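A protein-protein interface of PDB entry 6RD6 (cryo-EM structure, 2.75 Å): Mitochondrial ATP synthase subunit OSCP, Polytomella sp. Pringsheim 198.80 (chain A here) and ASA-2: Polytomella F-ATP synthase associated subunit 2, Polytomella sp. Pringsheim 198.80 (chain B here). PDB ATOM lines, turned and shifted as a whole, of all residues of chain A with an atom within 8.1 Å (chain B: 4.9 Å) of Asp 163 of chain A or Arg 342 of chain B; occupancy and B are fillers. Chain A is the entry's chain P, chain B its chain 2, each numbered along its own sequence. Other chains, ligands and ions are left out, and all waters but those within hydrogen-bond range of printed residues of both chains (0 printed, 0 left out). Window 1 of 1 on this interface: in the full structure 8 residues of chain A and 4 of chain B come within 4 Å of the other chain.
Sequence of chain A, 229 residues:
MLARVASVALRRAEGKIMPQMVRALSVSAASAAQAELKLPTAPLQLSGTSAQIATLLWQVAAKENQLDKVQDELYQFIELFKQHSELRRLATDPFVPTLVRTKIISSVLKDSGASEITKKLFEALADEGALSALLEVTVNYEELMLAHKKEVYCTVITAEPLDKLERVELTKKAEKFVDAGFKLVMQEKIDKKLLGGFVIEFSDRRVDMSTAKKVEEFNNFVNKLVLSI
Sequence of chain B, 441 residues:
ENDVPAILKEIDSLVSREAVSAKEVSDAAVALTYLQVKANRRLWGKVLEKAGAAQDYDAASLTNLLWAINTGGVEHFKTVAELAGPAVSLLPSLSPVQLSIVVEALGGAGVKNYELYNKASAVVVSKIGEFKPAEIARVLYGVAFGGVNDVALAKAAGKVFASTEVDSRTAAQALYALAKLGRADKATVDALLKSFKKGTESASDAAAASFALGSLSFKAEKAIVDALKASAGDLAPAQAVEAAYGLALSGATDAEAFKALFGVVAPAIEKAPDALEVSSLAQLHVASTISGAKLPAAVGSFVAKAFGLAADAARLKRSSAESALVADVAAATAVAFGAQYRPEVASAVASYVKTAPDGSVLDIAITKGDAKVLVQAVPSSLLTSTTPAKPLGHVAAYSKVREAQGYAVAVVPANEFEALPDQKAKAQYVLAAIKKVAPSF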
ATOM      1  N   THR A 158       9.988   7.363 -12.576  1.00  0.00           N
ATOM      2  CA  THR A 158      11.310   7.736 -12.106  1.00  0.00           C
ATOM      3  C   THR A 158      11.302   9.200 -11.698  1.00  0.00           C
ATOM      4  O   THR A 158      10.332   9.928 -11.919  1.00  0.00           O
ATOM      5  CB  THR A 158      12.381   7.496 -13.173  1.00  0.00           C
ATOM      6  OG1 THR A 158      11.976   8.115 -14.399  1.00  0.00           O
ATOM      7  CG2 THR A 158      12.578   6.006 -13.403  1.00  0.00           C
ATOM      8  N   ALA A 159      12.407   9.628 -11.090  1.00  0.00           N
ATOM      9  CA  ALA A 159      12.548  11.031 -10.719  1.00  0.00           C
ATOM     10  C   ALA A 159      12.938  11.873 -11.923  1.00  0.00           C
ATOM     11  O   ALA A 159      12.515  13.027 -12.054  1.00  0.00           O
ATOM     12  CB  ALA A 159      13.586  11.174  -9.609  1.00  0.00           C
ATOM     13  N   GLU A 160      13.740  11.309 -12.810  1.00  0.00           N
ATOM     14  CA  GLU A 160      14.360  12.003 -13.925  1.00  0.00           C
ATOM     15  C   GLU A 160      14.040  11.265 -15.213  1.00  0.00           C
ATOM     16  O   GLU A 160      13.666  10.087 -15.183  1.00  0.00           O
ATOM     17  CB  GLU A 160      15.879  12.077 -13.713  1.00  0.00           C
ATOM     18  CG  GLU A 160      16.289  12.930 -12.525  1.00  0.00           C
ATOM     19  CD  GLU A 160      17.777  12.878 -12.256  1.00  0.00           C
ATOM     20  OE1 GLU A 160      18.470  12.065 -12.904  1.00  0.00           O
ATOM     21  OE2 GLU A 160      18.254  13.645 -11.393  1.00  0.00           O
ATOM     22  N   PRO A 161      14.132  11.938 -16.359  1.00  0.00           N
ATOM     23  CA  PRO A 161      14.080  11.224 -17.639  1.00  0.00           C
ATOM     24  C   PRO A 161      15.251  10.263 -17.781  1.00  0.00           C
ATOM     25  O   PRO A 161      16.362  10.533 -17.322  1.00  0.00           O
ATOM     26  CB  PRO A 161      14.139  12.351 -18.673  1.00  0.00           C
ATOM     27  CG  PRO A 161      13.549  13.516 -17.971  1.00  0.00           C
ATOM     28  CD  PRO A 161      14.004  13.395 -16.546  1.00  0.00           C
ATOM     29  N   LEU A 162      14.989   9.130 -18.423  1.00  0.00           N
ATOM     30  CA  LEU A 162      15.914   8.007 -18.372  1.00  0.00           C
ATOM     31  C   LEU A 162      17.067   8.179 -19.352  1.00  0.00           C
ATOM     32  O   LEU A 162      16.887   8.653 -20.477  1.00  0.00           O
ATOM     33  CB  LEU A 162      15.175   6.708 -18.687  1.00  0.00           C
ATOM     34  CG  LEU A 162      14.502   5.906 -17.577  1.00  0.00           C
ATOM     35  CD1 LEU A 162      13.245   6.589 -17.084  1.00  0.00           C
ATOM     36  CD2 LEU A 162      14.169   4.535 -18.109  1.00  0.00           C
ATOM     37  N   ASP A 163      18.257   7.786 -18.913  1.00  0.00           N
ATOM     38  CA  ASP A 163      19.348   7.499 -19.826  1.00  0.00           C
ATOM     39  C   ASP A 163      19.132   6.115 -20.427  1.00  0.00           C
ATOM     40  O   ASP A 163      18.398   5.292 -19.880  1.00  0.00           O
ATOM     41  CB  ASP A 163      20.690   7.558 -19.097  1.00  0.00           C
ATOM     42  CG  ASP A 163      21.132   8.975 -18.805  1.00  0.00           C
ATOM     43  OD1 ASP A 163      22.079   9.151 -18.010  1.00  0.00           O
ATOM     44  OD2 ASP A 163      20.536   9.915 -19.369  1.00  0.00           O
ATOM     45  N   LYS A 164      19.780   5.857 -21.564  1.00  0.00           N
ATOM     46  CA  LYS A 164      19.542   4.593 -22.255  1.00  0.00           C
ATOM     47  C   LYS A 164      20.250   3.437 -21.553  1.00  0.00           C
ATOM     48  O   LYS A 164      19.740   2.308 -21.527  1.00  0.00           O
ATOM     49  CB  LYS A 164      19.952   4.701 -23.726  1.00  0.00           C
ATOM     50  CG  LYS A 164      21.397   5.059 -23.989  1.00  0.00           C
ATOM     51  CD  LYS A 164      21.719   4.919 -25.466  1.00  0.00           C
ATOM     52  CE  LYS A 164      21.647   3.471 -25.911  1.00  0.00           C
ATOM     53  NZ  LYS A 164      22.514   2.593 -25.081  1.00  0.00           N
ATOM     54  N   LEU A 165      21.409   3.703 -20.945  1.00  0.00           N
ATOM     55  CA  LEU A 165      22.036   2.688 -20.106  1.00  0.00           C
ATOM     56  C   LEU A 165      21.248   2.507 -18.815  1.00  0.00           C
ATOM     57  O   LEU A 165      21.102   1.382 -18.319  1.00  0.00           O
ATOM     58  CB  LEU A 165      23.493   3.062 -19.827  1.00  0.00           C
ATOM     59  CG  LEU A 165      24.440   2.026 -19.212  1.00  0.00           C
ATOM     60  CD1 LEU A 165      25.828   2.206 -19.795  1.00  0.00           C
ATOM     61  CD2 LEU A 165      24.516   2.139 -17.697  1.00  0.00           C
ATOM     62  N   GLU A 166      20.709   3.606 -18.280  1.00  0.00           N
ATOM     63  CA  GLU A 166      19.771   3.522 -17.166  1.00  0.00           C
ATOM     64  C   GLU A 166      18.512   2.768 -17.570  1.00  0.00           C
ATOM     65  O   GLU A 166      17.958   2.006 -16.771  1.00  0.00           O
ATOM     66  CB  GLU A 166      19.418   4.927 -16.680  1.00  0.00           C
ATOM     67  CG  GLU A 166      18.780   4.988 -15.307  1.00  0.00           C
ATOM     68  CD  GLU A 166      18.769   6.395 -14.740  1.00  0.00           C
ATOM     69  OE1 GLU A 166      18.337   6.572 -13.583  1.00  0.00           O
ATOM     70  OE2 GLU A 166      19.193   7.326 -15.456  1.00  0.00           O
ATOM     71  N   ARG A 167      18.081   2.931 -18.826  1.00  0.00           N
ATOM     72  CA  ARG A 167      16.895   2.233 -19.314  1.00  0.00           C
ATOM     73  C   ARG A 167      17.126   0.732 -19.405  1.00  0.00           C
ATOM     74  O   ARG A 167      16.269  -0.054 -18.989  1.00  0.00           O
ATOM     75  CB  ARG A 167      16.476   2.782 -20.674  1.00  0.00           C
ATOM     76  CG  ARG A 167      15.174   2.216 -21.192  1.00  0.00           C
ATOM     77  CD  ARG A 167      14.824   2.819 -22.533  1.00  0.00           C
ATOM     78  NE  ARG A 167      15.128   4.245 -22.578  1.00  0.00           N
ATOM     79  CZ  ARG A 167      14.289   5.196 -22.189  1.00  0.00           C
ATOM     80  NH1 ARG A 167      13.090   4.876 -21.726  1.00  0.00           N
ATOM     81  NH2 ARG A 167      14.647   6.470 -22.263  1.00  0.00           N
ATOM     82  N   VAL A 168      18.280   0.309 -19.927  1.00  0.00           N
ATOM     83  CA  VAL A 168      18.505  -1.127 -20.078  1.00  0.00           C
ATOM     84  C   VAL A 168      18.819  -1.771 -18.729  1.00  0.00           C
ATOM     85  O   VAL A 168      18.448  -2.928 -18.484  1.00  0.00           O
ATOM     86  CB  VAL A 168      19.588  -1.413 -21.140  1.00  0.00           C
ATOM     87  CG1 VAL A 168      19.141  -0.886 -22.496  1.00  0.00           C
ATOM     88  CG2 VAL A 168      20.932  -0.823 -20.767  1.00  0.00           C
ATOM     89  N   GLU A 169      19.436  -1.019 -17.807  1.00  0.00           N
ATOM     90  CA  GLU A 169      19.649  -1.550 -16.463  1.00  0.00           C
ATOM     91  C   GLU A 169      18.335  -1.665 -15.697  1.00  0.00           C
ATOM     92  O   GLU A 169      18.114  -2.646 -14.979  1.00  0.00           O
ATOM     93  CB  GLU A 169      20.638  -0.676 -15.696  1.00  0.00           C
ATOM     94  CG  GLU A 169      22.081  -1.138 -15.807  1.00  0.00           C
ATOM     95  CD  GLU A 169      23.044  -0.226 -15.072  1.00  0.00           C
ATOM     96  OE1 GLU A 169      22.583   0.772 -14.480  1.00  0.00           O
ATOM     97  OE2 GLU A 169      24.260  -0.510 -15.083  1.00  0.00           O
ATOM     98  N   LEU A 170      17.434  -0.696 -15.879  1.00  0.00           N
ATOM     99  CA  LEU A 170      16.123  -0.762 -15.245  1.00  0.00           C
ATOM    100  C   LEU A 170      15.269  -1.864 -15.855  1.00  0.00           C
ATOM    101  O   LEU A 170      14.489  -2.513 -15.149  1.00  0.00           O
ATOM    102  CB  LEU A 170      15.442   0.601 -15.365  1.00  0.00           C
ATOM    103  CG  LEU A 170      13.955   0.848 -15.120  1.00  0.00           C
ATOM    104  CD1 LEU A 170      13.469   0.294 -13.804  1.00  0.00           C
ATOM    105  CD2 LEU A 170      13.741   2.338 -15.152  1.00  0.00           C
ATOM    106  N   GLU A 188       6.950   5.384 -19.223  1.00  0.00           N
ATOM    107  CA  GLU A 188       7.765   6.208 -18.340  1.00  0.00           C
ATOM    108  C   GLU A 188       6.950   7.395 -17.847  1.00  0.00           C
ATOM    109  O   GLU A 188       6.227   8.024 -18.626  1.00  0.00           O
ATOM    110  CB  GLU A 188       9.030   6.685 -19.051  1.00  0.00           C
ATOM    111  CG  GLU A 188      10.113   5.629 -19.158  1.00  0.00           C
ATOM    112  CD  GLU A 188       9.974   4.775 -20.396  1.00  0.00           C
ATOM    113  OE1 GLU A 188       9.065   5.046 -21.205  1.00  0.00           O
ATOM    114  OE2 GLU A 188      10.774   3.830 -20.559  1.00  0.00           O
ATOM    115  N   GLN B 340      29.133   9.271 -20.119  1.00  0.00           N
ATOM    116  CA  GLN B 340      28.047  10.128 -20.572  1.00  0.00           C
ATOM    117  C   GLN B 340      26.692   9.716 -20.016  1.00  0.00           C
ATOM    118  O   GLN B 340      25.700  10.404 -20.270  1.00  0.00           O
ATOM    119  CB  GLN B 340      27.992  10.141 -22.103  1.00  0.00           C
ATOM    120  CG  GLN B 340      27.567   8.821 -22.721  1.00  0.00           C
ATOM    121  CD  GLN B 340      28.743   7.923 -23.047  1.00  0.00           C
ATOM    122  OE1 GLN B 340      29.875   8.190 -22.644  1.00  0.00           O
ATOM    123  NE2 GLN B 340      28.480   6.845 -23.773  1.00  0.00           N
ATOM    124  N   TYR B 341      26.625   8.621 -19.266  1.00  0.00           N
ATOM    125  CA  TYR B 341      25.387   8.155 -18.661  1.00  0.00           C
ATOM    126  C   TYR B 341      25.550   8.124 -17.150  1.00  0.00           C
ATOM    127  O   TYR B 341      26.632   7.813 -16.642  1.00  0.00           O
ATOM    128  CB  TYR B 341      25.002   6.768 -19.183  1.00  0.00           C
ATOM    129  CG  TYR B 341      24.868   6.707 -20.686  1.00  0.00           C
ATOM    130  CD1 TYR B 341      24.180   7.693 -21.380  1.00  0.00           C
ATOM    131  CD2 TYR B 341      25.442   5.672 -21.411  1.00  0.00           C
ATOM    132  CE1 TYR B 341      24.061   7.645 -22.754  1.00  0.00           C
ATOM    133  CE2 TYR B 341      25.329   5.615 -22.786  1.00  0.00           C
ATOM    134  CZ  TYR B 341      24.637   6.604 -23.450  1.00  0.00           C
ATOM    135  OH  TYR B 341      24.524   6.550 -24.819  1.00  0.00           O
ATOM    136  N   ARG B 342      24.467   8.448 -16.442  1.00  0.00           N
ATOM    137  CA  ARG B 342      24.423   8.589 -14.987  1.00  0.00           C
ATOM    138  C   ARG B 342      24.872   7.367 -14.175  1.00  0.00           C
ATOM    139  O   ARG B 342      25.549   7.570 -13.156  1.00  0.00           O
ATOM    140  CB  ARG B 342      23.016   9.018 -14.557  1.00  0.00           C
ATOM    141  CG  ARG B 342      22.664  10.443 -14.929  1.00  0.00           C
ATOM    142  CD  ARG B 342      21.425  10.909 -14.191  1.00  0.00           C
ATOM    143  NE  ARG B 342      20.243  10.153 -14.594  1.00  0.00           N
ATOM    144  CZ  ARG B 342      19.409  10.533 -15.554  1.00  0.00           C
ATOM    145  NH1 ARG B 342      18.360   9.784 -15.859  1.00  0.00           N
ATOM    146  NH2 ARG B 342      19.624  11.664 -16.209  1.00  0.00           N
ATOM    147  N   PRO B 343      24.544   6.104 -14.530  1.00  0.00           N
ATOM    148  CA  PRO B 343      25.157   4.992 -13.777  1.00  0.00           C
ATOM    149  C   PRO B 343      26.657   4.867 -13.984  1.00  0.00           C
ATOM    150  O   PRO B 343      27.378   4.513 -13.044  1.00  0.00           O
ATOM    151  CB  PRO B 343      24.399   3.764 -14.296  1.00  0.00           C
ATOM    152  CG  PRO B 343      23.116   4.290 -14.752  1.00  0.00           C
ATOM    153  CD  PRO B 343      23.475   5.574 -15.404  1.00  0.00           C
ATOM    154  N   GLU B 344      27.148   5.177 -15.188  1.00  0.00           N
ATOM    155  CA  GLU B 344      28.588   5.180 -15.427  1.00  0.00           C
ATOM    156  C   GLU B 344      29.273   6.287 -14.640  1.00  0.00           C
ATOM    157  O   GLU B 344      30.362   6.084 -14.088  1.00  0.00           O
ATOM    158  CB  GLU B 344      28.874   5.341 -16.920  1.00  0.00           C
ATOM    159  CG  GLU B 344      28.404   4.190 -17.780  1.00  0.00           C
ATOM    160  CD  GLU B 344      28.981   4.250 -19.177  1.00  0.00           C
ATOM    161  OE1 GLU B 344      30.125   3.788 -19.367  1.00  0.00           O
ATOM    162  OE2 GLU B 344      28.295   4.764 -20.085  1.00  0.00           O
ATOM    163  N   VAL B 345      28.632   7.457 -14.559  1.00  0.00           N
ATOM    164  CA  VAL B 345      29.176   8.581 -13.798  1.00  0.00           C
ATOM    165  C   VAL B 345      29.222   8.243 -12.312  1.00  0.00           C
ATOM    166  O   VAL B 345      30.231   8.479 -11.640  1.00  0.00           O
ATOM    167  CB  VAL B 345      28.353   9.855 -14.068  1.00  0.00           C
ATOM    168  CG1 VAL B 345      28.733  10.970 -13.113  1.00  0.00           C
ATOM    169  CG2 VAL B 345      28.548  10.309 -15.497  1.00  0.00           C
ATOM    170  N   ALA B 346      28.146   7.641 -11.793  1.00  0.00           N
ATOM    171  CA  ALA B 346      28.102   7.276 -10.378  1.00  0.00           C
ATOM    172  C   ALA B 346      29.106   6.177 -10.047  1.00  0.00           C
ATOM    173  O   ALA B 346      29.750   6.215  -8.990  1.00  0.00           O
ATOM    174  CB  ALA B 346      26.690   6.841  -9.995  1.00  0.00           C
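Printed residues of chain B within 4 Å of Pro 161 of chain A: Arg 342.
Asp 163 of chain A touches two residues of chain B.
Printed residues of chain B within 4 Å of Glu 166 of chain A: Arg 342.
Glu 188 of chain A touches none of the printed residues of chain B.
Pro 343 of chain B touches just these residues of chain A: Leu 165 and Glu 169.
Ala 346 of chain B touches none of the printed residues of chain A.
The nearest residue of chain B that does not touch Asp 163 of chain A is Gln 340 of chain B (4.4 Å).
The nearest residue of chain A that does not touch Arg 342 of chain B is Leu 165 of chain A (6.3 Å).
Of the 14 printed residues of chain A, 8 touch a printed residue of chain B.
Hydrophobic or aromatic side chains of chain A that line the printed part of chain B: Leu 165.
Among the printed residues, 11 pairs touch across the chains.
Among the printed residues, Asp or Glu carboxylates within 4 Å of a Lys or Arg side-chain nitrogen of the other chain: Glu 160 of chain A with Arg 342 of chain B (3.1 Å), Asp 163 of chain A with Arg 342 of chain B (3.7 Å) and Glu 166 of chain A with Arg 342 of chain B (2.6 Å).
NE of Arg 342 of chain B is in salt-bridge range of OE1 of Glu 160 of chain A (3.1 Å).
NH1 of Arg 342 of chain B is in hydrogen-bond range of O of Pro 161 of chain A.
The guanidinium group (NH2) of Arg 342 of chain B lies within salt-bridge range of the side-chain carboxylate (OD2) of Asp 163 of chain A, at 3.7 Å.
The guanidinium group of Arg 342 of chain B is in salt-bridge range of the side-chain carboxylate of Glu 166 of chain A, 2.6 Å away.
OG1 of Thr 158 of chain A lies within hydrogen-bond range of O of Glu 160 of chain A, at 2.7 Å.
Among the printed residues, merely in contact across the chains: Lys 164 of chain A with Tyr 341 of chain B (3.3 Å), Glu 169 of chain A with Pro 343 of chain B (3.5 Å), Asp 163 of chain A with Tyr 341 of chain B (3.5 Å), Leu 165 of chain A with Glu 344 of chain B (3.6 Å), Leu 165 of chain A with Tyr 341 of chain B (3.6 Å), Leu 165 of chain A with Pro 343 of chain B (3.8 Å) and Leu 162 of chain A with Arg 342 of chain B (3.9 Å).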
